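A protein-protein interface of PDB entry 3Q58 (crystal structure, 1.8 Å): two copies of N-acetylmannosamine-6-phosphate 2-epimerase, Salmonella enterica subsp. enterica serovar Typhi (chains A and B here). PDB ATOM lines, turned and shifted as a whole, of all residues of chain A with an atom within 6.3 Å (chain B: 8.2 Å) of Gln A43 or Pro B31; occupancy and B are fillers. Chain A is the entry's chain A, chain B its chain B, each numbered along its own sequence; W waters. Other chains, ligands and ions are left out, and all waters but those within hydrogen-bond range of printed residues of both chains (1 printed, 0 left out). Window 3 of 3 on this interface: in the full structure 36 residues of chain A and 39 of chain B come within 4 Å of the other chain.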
ATOM      1  N   CYS A  24     -39.520  21.318 -18.353  1.00  0.00           N
ATOM      2  CA  CYS A  24     -38.301  21.801 -18.899  1.00  0.00           C
ATOM      3  C   CYS A  24     -38.440  22.629 -20.158  1.00  0.00           C
ATOM      4  O   CYS A  24     -37.990  22.250 -21.165  1.00  0.00           O
ATOM      5  CB  CYS A  24     -37.292  20.694 -19.077  1.00  0.00           C
ATOM      6  SG  CYS A  24     -36.984  19.745 -17.574  1.00  0.00           S
ATOM      7  N   GLU A  36     -29.695  20.208 -26.198  1.00  0.00           N
ATOM      8  CA  GLU A  36     -28.771  19.598 -25.245  1.00  0.00           C
ATOM      9  C   GLU A  36     -28.925  20.198 -23.843  1.00  0.00           C
ATOM     10  O   GLU A  36     -28.706  19.524 -22.835  1.00  0.00           O
ATOM     11  CB  GLU A  36     -27.320  19.745 -25.712  1.00  0.00           C
ATOM     12  CG  GLU A  36     -27.032  19.130 -27.072  1.00  0.00           C
ATOM     13  CD  GLU A  36     -27.281  20.095 -28.228  1.00  0.00           C
ATOM     14  OE1 GLU A  36     -28.112  21.022 -28.085  1.00  0.00           O
ATOM     15  OE2 GLU A  36     -26.632  19.928 -29.286  1.00  0.00           O
ATOM     16  N   VAL A  38     -31.847  21.608 -22.732  1.00  0.00           N
ATOM     17  CA  VAL A  38     -33.123  21.056 -22.275  1.00  0.00           C
ATOM     18  C   VAL A  38     -32.896  19.650 -21.711  1.00  0.00           C
ATOM     19  O   VAL A  38     -33.367  19.325 -20.623  1.00  0.00           O
ATOM     20  CB  VAL A  38     -34.195  21.072 -23.383  1.00  0.00           C
ATOM     21  CG1 VAL A  38     -35.450  20.346 -22.921  1.00  0.00           C
ATOM     22  CG2 VAL A  38     -34.517  22.510 -23.775  1.00  0.00           C
ATOM     23  N   ALA A  39     -32.130  18.836 -22.430  1.00  0.00           N
ATOM     24  CA  ALA A  39     -31.775  17.503 -21.956  1.00  0.00           C
ATOM     25  C   ALA A  39     -31.076  17.539 -20.595  1.00  0.00           C
ATOM     26  O   ALA A  39     -31.393  16.751 -19.707  1.00  0.00           O
ATOM     27  CB  ALA A  39     -30.898  16.791 -22.976  1.00  0.00           C
ATOM     28  N   ALA A  40     -30.102  18.436 -20.450  1.00  0.00           N
ATOM     29  CA  ALA A  40     -29.367  18.561 -19.200  1.00  0.00           C
ATOM     30  C   ALA A  40     -30.282  18.953 -18.036  1.00  0.00           C
ATOM     31  O   ALA A  40     -30.129  18.439 -16.928  1.00  0.00           O
ATOM     32  CB  ALA A  40     -28.224  19.557 -19.349  1.00  0.00           C
ATOM     33  N   MET A  41     -31.234  19.851 -18.283  1.00  0.00           N
ATOM     34  CA  MET A  41     -32.153  20.266 -17.216  1.00  0.00           C
ATOM     35  C   MET A  41     -33.002  19.095 -16.754  1.00  0.00           C
ATOM     36  O   MET A  41     -33.232  18.925 -15.558  1.00  0.00           O
ATOM     37  CB  MET A  41     -33.108  21.385 -17.659  1.00  0.00           C
ATOM     38  CG  MET A  41     -32.665  22.218 -18.837  1.00  0.00           C
ATOM     39  SD  MET A  41     -33.927  23.686 -19.129  1.00  0.00           S
ATOM     40  CE  MET A  41     -33.326  24.755 -17.730  1.00  0.00           C
ATOM     41  N   ALA A  42     -33.479  18.306 -17.715  1.00  0.00           N
ATOM     42  CA  ALA A  42     -34.349  17.170 -17.423  1.00  0.00           C
ATOM     43  C   ALA A  42     -33.626  16.135 -16.577  1.00  0.00           C
ATOM     44  O   ALA A  42     -34.180  15.615 -15.615  1.00  0.00           O
ATOM     45  CB  ALA A  42     -34.872  16.533 -18.724  1.00  0.00           C
ATOM     46  N   GLN A  43     -32.381  15.841 -16.949  1.00  0.00           N
ATOM     47  CA  GLN A  43     -31.540  14.914 -16.198  1.00  0.00           C
ATOM     48  C   GLN A  43     -31.260  15.430 -14.794  1.00  0.00           C
ATOM     49  O   GLN A  43     -31.335  14.681 -13.829  1.00  0.00           O
ATOM     50  CB  GLN A  43     -30.226  14.674 -16.939  1.00  0.00           C
ATOM     51  CG  GLN A  43     -30.434  13.937 -18.257  1.00  0.00           C
ATOM     52  CD  GLN A  43     -29.158  13.795 -19.058  1.00  0.00           C
ATOM     53  OE1 GLN A  43     -28.834  14.646 -19.884  1.00  0.00           O
ATOM     54  NE2 GLN A  43     -28.428  12.711 -18.822  1.00  0.00           N
ATOM     55  N   ALA A  44     -30.936  16.712 -14.690  1.00  0.00           N
ATOM     56  CA  ALA A  44     -30.694  17.328 -13.393  1.00  0.00           C
ATOM     57  C   ALA A  44     -31.933  17.261 -12.502  1.00  0.00           C
ATOM     58  O   ALA A  44     -31.852  16.812 -11.363  1.00  0.00           O
ATOM     59  CB  ALA A  44     -30.205  18.754 -13.551  1.00  0.00           C
ATOM     60  N   ALA A  45     -33.088  17.663 -13.031  1.00  0.00           N
ATOM     61  CA  ALA A  45     -34.323  17.574 -12.255  1.00  0.00           C
ATOM     62  C   ALA A  45     -34.641  16.139 -11.809  1.00  0.00           C
ATOM     63  O   ALA A  45     -35.034  15.915 -10.661  1.00  0.00           O
ATOM     64  CB  ALA A  45     -35.493  18.159 -13.037  1.00  0.00           C
ATOM     65  N   ALA A  46     -34.472  15.171 -12.708  1.00  0.00           N
ATOM     66  CA  ALA A  46     -34.795  13.783 -12.379  1.00  0.00           C
ATOM     67  C   ALA A  46     -33.836  13.220 -11.335  1.00  0.00           C
ATOM     68  O   ALA A  46     -34.172  12.279 -10.621  1.00  0.00           O
ATOM     69  CB  ALA A  46     -34.800  12.905 -13.634  1.00  0.00           C
ATOM     70  N   SER A  47     -32.641  13.794 -11.253  1.00  0.00           N
ATOM     71  CA  SER A  47     -31.659  13.339 -10.282  1.00  0.00           C
ATOM     72  C   SER A  47     -31.957  13.914  -8.896  1.00  0.00           C
ATOM     73  O   SER A  47     -31.405  13.459  -7.892  1.00  0.00           O
ATOM     74  CB  SER A  47     -30.242  13.728 -10.716  1.00  0.00           C
ATOM     75  OG  SER A  47     -29.943  15.063 -10.338  1.00  0.00           O
ATOM     76  N   ALA A  48     -32.844  14.901  -8.844  1.00  0.00           N
ATOM     77  CA  ALA A  48     -33.040  15.667  -7.621  1.00  0.00           C
ATOM     78  C   ALA A  48     -34.492  15.766  -7.170  1.00  0.00           C
ATOM     79  O   ALA A  48     -34.859  16.718  -6.487  1.00  0.00           O
ATOM     80  CB  ALA A  48     -32.438  17.061  -7.773  1.00  0.00           C
ATOM     81  N   VAL A  53     -40.920  14.563 -16.161  1.00  0.00           N
ATOM     82  CA  VAL A  53     -40.682  15.883 -16.730  1.00  0.00           C
ATOM     83  C   VAL A  53     -41.671  16.177 -17.857  1.00  0.00           C
ATOM     84  O   VAL A  53     -42.216  15.256 -18.470  1.00  0.00           O
ATOM     85  CB  VAL A  53     -39.247  16.013 -17.281  1.00  0.00           C
ATOM     86  CG1 VAL A  53     -38.216  15.886 -16.139  1.00  0.00           C
ATOM     87  CG2 VAL A  53     -39.003  14.964 -18.375  1.00  0.00           C
ATOM     88  N   VAL A  64     -33.558  14.407 -25.350  1.00  0.00           N
ATOM     89  CA  VAL A  64     -33.767  14.042 -23.950  1.00  0.00           C
ATOM     90  C   VAL A  64     -33.917  12.530 -23.734  1.00  0.00           C
ATOM     91  O   VAL A  64     -33.293  11.952 -22.841  1.00  0.00           O
ATOM     92  CB  VAL A  64     -35.070  14.710 -23.423  1.00  0.00           C
ATOM     93  CG1 VAL A  64     -35.512  14.093 -22.114  1.00  0.00           C
ATOM     94  CG2 VAL A  64     -34.898  16.217 -23.286  1.00  0.00           C
ATOM     95  N   HIS A  67     -31.437   9.533 -22.623  1.00  0.00           N
ATOM     96  CA  HIS A  67     -30.630   9.759 -21.434  1.00  0.00           C
ATOM     97  C   HIS A  67     -31.476  10.022 -20.194  1.00  0.00           C
ATOM     98  O   HIS A  67     -30.972  10.523 -19.188  1.00  0.00           O
ATOM     99  CB  HIS A  67     -29.682  10.937 -21.672  1.00  0.00           C
ATOM    100  CG  HIS A  67     -28.857  10.802 -22.914  1.00  0.00           C
ATOM    101  ND1 HIS A  67     -28.084   9.691 -23.178  1.00  0.00           N
ATOM    102  CD2 HIS A  67     -28.689  11.636 -23.969  1.00  0.00           C
ATOM    103  CE1 HIS A  67     -27.474   9.845 -24.340  1.00  0.00           C
ATOM    104  NE2 HIS A  67     -27.823  11.018 -24.841  1.00  0.00           N
ATOM    105  N   LEU A  68     -32.760   9.684 -20.260  1.00  0.00           N
ATOM    106  CA  LEU A  68     -33.670   9.980 -19.160  1.00  0.00           C
ATOM    107  C   LEU A  68     -34.509   8.755 -18.818  1.00  0.00           C
ATOM    108  O   LEU A  68     -35.137   8.161 -19.696  1.00  0.00           O
ATOM    109  CB  LEU A  68     -34.582  11.155 -19.534  1.00  0.00           C
ATOM    110  CG  LEU A  68     -35.361  11.786 -18.381  1.00  0.00           C
ATOM    111  CD1 LEU A  68     -34.411  12.522 -17.462  1.00  0.00           C
ATOM    112  CD2 LEU A  68     -36.420  12.731 -18.920  1.00  0.00           C
ATOM    113  N   PRO B  26     -23.184  25.926 -11.231  1.00  0.00           N
ATOM    114  CA  PRO B  26     -24.039  24.744 -11.093  1.00  0.00           C
ATOM    115  C   PRO B  26     -23.395  23.745 -10.146  1.00  0.00           C
ATOM    116  O   PRO B  26     -22.220  23.889  -9.812  1.00  0.00           O
ATOM    117  CB  PRO B  26     -24.090  24.175 -12.517  1.00  0.00           C
ATOM    118  CG  PRO B  26     -22.839  24.646 -13.168  1.00  0.00           C
ATOM    119  CD  PRO B  26     -22.497  25.977 -12.533  1.00  0.00           C
ATOM    120  N   VAL B  27     -24.154  22.746  -9.715  1.00  0.00           N
ATOM    121  CA  VAL B  27     -23.604  21.711  -8.848  1.00  0.00           C
ATOM    122  C   VAL B  27     -22.465  21.019  -9.591  1.00  0.00           C
ATOM    123  O   VAL B  27     -22.638  20.596 -10.732  1.00  0.00           O
ATOM    124  CB  VAL B  27     -24.697  20.690  -8.501  1.00  0.00           C
ATOM    125  CG1 VAL B  27     -24.105  19.504  -7.756  1.00  0.00           C
ATOM    126  CG2 VAL B  27     -25.808  21.370  -7.702  1.00  0.00           C
ATOM    127  N   PRO B  28     -21.281  20.921  -8.969  1.00  0.00           N
ATOM    128  CA  PRO B  28     -20.198  20.294  -9.739  1.00  0.00           C
ATOM    129  C   PRO B  28     -20.515  18.857 -10.124  1.00  0.00           C
ATOM    130  O   PRO B  28     -21.022  18.080  -9.312  1.00  0.00           O
ATOM    131  CB  PRO B  28     -18.984  20.366  -8.787  1.00  0.00           C
ATOM    132  CG  PRO B  28     -19.526  20.771  -7.449  1.00  0.00           C
ATOM    133  CD  PRO B  28     -20.808  21.507  -7.703  1.00  0.00           C
ATOM    134  N   GLY B  29     -20.231  18.510 -11.374  1.00  0.00           N
ATOM    135  CA  GLY B  29     -20.532  17.183 -11.872  1.00  0.00           C
ATOM    136  C   GLY B  29     -21.942  17.050 -12.425  1.00  0.00           C
ATOM    137  O   GLY B  29     -22.266  16.050 -13.064  1.00  0.00           O
ATOM    138  N   SER B  30     -22.779  18.052 -12.167  1.00  0.00           N
ATOM    139  CA  SER B  30     -24.164  18.079 -12.656  1.00  0.00           C
ATOM    140  C   SER B  30     -24.230  18.041 -14.181  1.00  0.00           C
ATOM    141  O   SER B  30     -23.298  18.478 -14.850  1.00  0.00           O
ATOM    142  CB  SER B  30     -24.862  19.348 -12.157  1.00  0.00           C
ATOM    143  OG  SER B  30     -26.078  19.592 -12.850  1.00  0.00           O
ATOM    144  N   PRO B  31     -25.342  17.532 -14.739  1.00  0.00           N
ATOM    145  CA  PRO B  31     -25.515  17.652 -16.191  1.00  0.00           C
ATOM    146  C   PRO B  31     -25.407  19.106 -16.640  1.00  0.00           C
ATOM    147  O   PRO B  31     -25.036  19.372 -17.782  1.00  0.00           O
ATOM    148  CB  PRO B  31     -26.938  17.134 -16.411  1.00  0.00           C
ATOM    149  CG  PRO B  31     -27.134  16.138 -15.314  1.00  0.00           C
ATOM    150  CD  PRO B  31     -26.387  16.693 -14.124  1.00  0.00           C
ATOM    151  N   MET B  32     -25.735  20.031 -15.743  1.00  0.00           N
ATOM    152  CA  MET B  32     -25.653  21.465 -16.035  1.00  0.00           C
ATOM    153  C   MET B  32     -24.217  21.988 -15.963  1.00  0.00           C
ATOM    154  O   MET B  32     -23.920  23.102 -16.418  1.00  0.00           O
ATOM    155  CB  MET B  32     -26.533  22.263 -15.061  1.00  0.00           C
ATOM    156  CG  MET B  32     -28.000  21.868 -15.080  1.00  0.00           C
ATOM    157  SD  MET B  32     -28.822  22.163 -16.827  1.00  0.00           S
ATOM    158  CE  MET B  32     -28.945  24.097 -16.764  1.00  0.00           C
ATOM    159  N   ASP B  33     -23.324  21.197 -15.380  1.00  0.00           N
ATOM    160  CA  ASP B  33     -21.955  21.653 -15.163  1.00  0.00           C
ATOM    161  C   ASP B  33     -21.091  21.440 -16.404  1.00  0.00           C
ATOM    162  O   ASP B  33     -20.229  20.557 -16.429  1.00  0.00           O
ATOM    163  CB  ASP B  33     -21.329  20.979 -13.932  1.00  0.00           C
ATOM    164  CG  ASP B  33     -19.936  21.489 -13.634  1.00  0.00           C
ATOM    165  OD1 ASP B  33     -19.604  22.610 -14.081  1.00  0.00           O
ATOM    166  OD2 ASP B  33     -19.176  20.779 -12.934  1.00  0.00           O
ATOM    167  N   LYS B  34     -21.355  22.247 -17.431  1.00  0.00           N
ATOM    168  CA  LYS B  34     -20.524  22.320 -18.631  1.00  0.00           C
ATOM    169  C   LYS B  34     -20.303  23.793 -18.943  1.00  0.00           C
ATOM    170  O   LYS B  34     -21.203  24.609 -18.747  1.00  0.00           O
ATOM    171  CB  LYS B  34     -21.205  21.629 -19.820  1.00  0.00           C
ATOM    172  CG  LYS B  34     -21.461  20.139 -19.616  1.00  0.00           C
ATOM    173  CD  LYS B  34     -22.269  19.552 -20.770  1.00  0.00           C
ATOM    174  CE  LYS B  34     -21.583  19.783 -22.113  1.00  0.00           C
ATOM    175  NZ  LYS B  34     -20.269  19.089 -22.208  1.00  0.00           N
ATOM    176  N   PRO B  35     -19.103  24.148 -19.427  1.00  0.00           N
ATOM    177  CA  PRO B  35     -18.781  25.565 -19.647  1.00  0.00           C
ATOM    178  C   PRO B  35     -19.754  26.271 -20.598  1.00  0.00           C
ATOM    179  O   PRO B  35     -20.084  27.441 -20.386  1.00  0.00           O
ATOM    180  CB  PRO B  35     -17.374  25.511 -20.257  1.00  0.00           C
ATOM    181  CG  PRO B  35     -16.809  24.219 -19.777  1.00  0.00           C
ATOM    182  CD  PRO B  35     -17.965  23.269 -19.744  1.00  0.00           C
ATOM    183  N   ILE B  37     -22.870  25.620 -20.908  1.00  0.00           N
ATOM    184  CA  ILE B  37     -24.128  25.815 -20.196  1.00  0.00           C
ATOM    185  C   ILE B  37     -23.980  26.952 -19.188  1.00  0.00           C
ATOM    186  O   ILE B  37     -24.852  27.802 -19.069  1.00  0.00           O
ATOM    187  CB  ILE B  37     -24.623  24.504 -19.527  1.00  0.00           C
ATOM    188  CG1 ILE B  37     -24.881  23.445 -20.602  1.00  0.00           C
ATOM    189  CG2 ILE B  37     -25.890  24.749 -18.705  1.00  0.00           C
ATOM    190  CD1 ILE B  37     -25.361  22.112 -20.062  1.00  0.00           C
ATOM    191  N   VAL B  38     -22.859  26.980 -18.480  1.00  0.00           N
ATOM    192  CA  VAL B  38     -22.569  28.109 -17.603  1.00  0.00           C
ATOM    193  C   VAL B  38     -22.641  29.407 -18.402  1.00  0.00           C
ATOM    194  O   VAL B  38     -23.219  30.398 -17.946  1.00  0.00           O
ATOM    195  CB  VAL B  38     -21.190  27.971 -16.940  1.00  0.00           C
ATOM    196  CG1 VAL B  38     -20.816  29.267 -16.216  1.00  0.00           C
ATOM    197  CG2 VAL B  38     -21.198  26.798 -15.979  1.00  0.00           C
ATOM    198  N   ILE B 216     -30.210  23.877 -10.443  1.00  0.00           N
ATOM    199  CA  ILE B 216     -31.491  23.181 -10.641  1.00  0.00           C
ATOM    200  C   ILE B 216     -31.717  22.113  -9.568  1.00  0.00           C
ATOM    201  O   ILE B 216     -32.820  21.987  -9.041  1.00  0.00           O
ATOM    202  CB  ILE B 216     -31.616  22.573 -12.062  1.00  0.00           C
ATOM    203  CG1 ILE B 216     -31.812  23.689 -13.097  1.00  0.00           C
ATOM    204  CG2 ILE B 216     -32.833  21.638 -12.160  1.00  0.00           C
ATOM    205  CD1 ILE B 216     -32.108  23.199 -14.514  1.00  0.00           C
ATOM    206  N   GLU B 217     -30.668  21.371  -9.225  1.00  0.00           N
ATOM    207  CA  GLU B 217     -30.794  20.316  -8.217  1.00  0.00           C
ATOM    208  C   GLU B 217     -31.203  20.883  -6.859  1.00  0.00           C
ATOM    209  O   GLU B 217     -32.016  20.281  -6.161  1.00  0.00           O
ATOM    210  CB  GLU B 217     -29.504  19.509  -8.079  1.00  0.00           C
ATOM    211  CG  GLU B 217     -29.157  18.667  -9.303  1.00  0.00           C
ATOM    212  CD  GLU B 217     -28.295  19.413 -10.307  1.00  0.00           C
ATOM    213  OE1 GLU B 217     -28.249  20.666 -10.261  1.00  0.00           O
ATOM    214  OE2 GLU B 217     -27.658  18.736 -11.143  1.00  0.00           O
ATOM    215  N   CYS B 220     -34.933  22.008  -7.155  1.00  0.00           N
ATOM    216  CA  CYS B 220     -35.767  20.811  -7.133  1.00  0.00           C
ATOM    217  C   CYS B 220     -35.901  20.235  -5.726  1.00  0.00           C
ATOM    218  O   CYS B 220     -36.983  19.798  -5.333  1.00  0.00           O
ATOM    219  CB  CYS B 220     -35.230  19.757  -8.102  1.00  0.00           C
ATOM    220  SG  CYS B 220     -35.542  20.183  -9.794  1.00  0.00           S
HETATM  221  O   HOH W   1     -27.554  16.090 -10.947  1.00  0.00           O
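Among the printed residues, merely in contact across the chains: Ala A40 with Pro B31, Ala A40 with Met B32, Ala A40 with Ile B37, Met A41 with Ile B216, Gln A43 with Pro B31, Ala A44 with Pro B31, Ala A44 with Glu B217, Ala A45 with Cys B220, Ser A47 with Glu B217, Ala A48 with Glu B217 and Ala A48 with Cys B220.
The backbone carbonyl oxygen (O) of Ala A39 lies close to the side-chain amide oxygen (OE1) of Gln A43. O of Ile B216 lies within hydrogen-bond range of SG of Cys B220 (3.4 Å). The side-chain hydroxyl (OG) of Ser B30 is in hydrogen-bond range of the side-chain carboxylate (OE2) of Glu B217 (2.5 Å). OG of Ser B30 lies close to N of Met B32 (2.9 Å). The side-chain amide nitrogen of Gln A43 is in hydrogen-bond range of the backbone carbonyl oxygen of His A67, at 3.4 Å. The backbone carbonyl oxygen (O) of Ala A44 sits at hydrogen-bond distance from the side-chain hydroxyl (OG) of Ser A47.
Of the 15 printed residues of chain B, 6 touch a printed residue of chain A. Hydrophobic or aromatic side chains of chain B that line the printed part of chain A: Pro B31, Met B32, Ile B37 and Ile B216. Of the 17 printed residues of chain A, 7 touch a printed residue of chain B. Printed residues of chain A that touch a printed residue of chain B: Ala A40, Met A41, Gln A43, Ala A44, Ala A45, Ser A47 and Ala A48. Among the printed residues, 12 pairs touch across the chains. Among the printed residues, no Asp or Glu carboxylate lies within 4 Å of a Lys or Arg side-chain nitrogen of the other chain.
Position printed for both chains: 38. Of the 12 pairs that touch across the chains among the printed residues, none has its exchanged pair printed and touching as well.
Gln A43 touches just one residue of chain B: Pro B31. Of chain A, only Ala A40 (3.5 Å), Gln A43 (3.8 Å) and Ala A44 (3.9 Å) come within 4 Å of Pro B31. Ala A40 touches three residues of chain B. Ala A42 touches none of the printed residues of chain B. Of chain B, only Pro B31 and Glu B217 come within 4 Å of Ala A44. Printed residues of chain A within 4 Å of Glu B217: Ala A44 (3.5 Å), Ser A47 (3.8 Å) and Ala A48 (3.6 Å). Of the printed residues of chain B, Ala A48 touches Glu B217 and Cys B220. The nearest residue of chain B that does not touch Gln A43 is Glu B217 (6.1 Å). The nearest printed residue of chain A that does not touch Pro B31 is Met A41 (5.4 Å).
N of Met A41 lies within hydrogen-bond range of SD of Met B32.
Water W1 lies within hydrogen-bond range of the side-chain carboxylate of Glu B217 (2.7 Å) and the side-chain hydroxyl of Ser A47 (2.7 Å).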
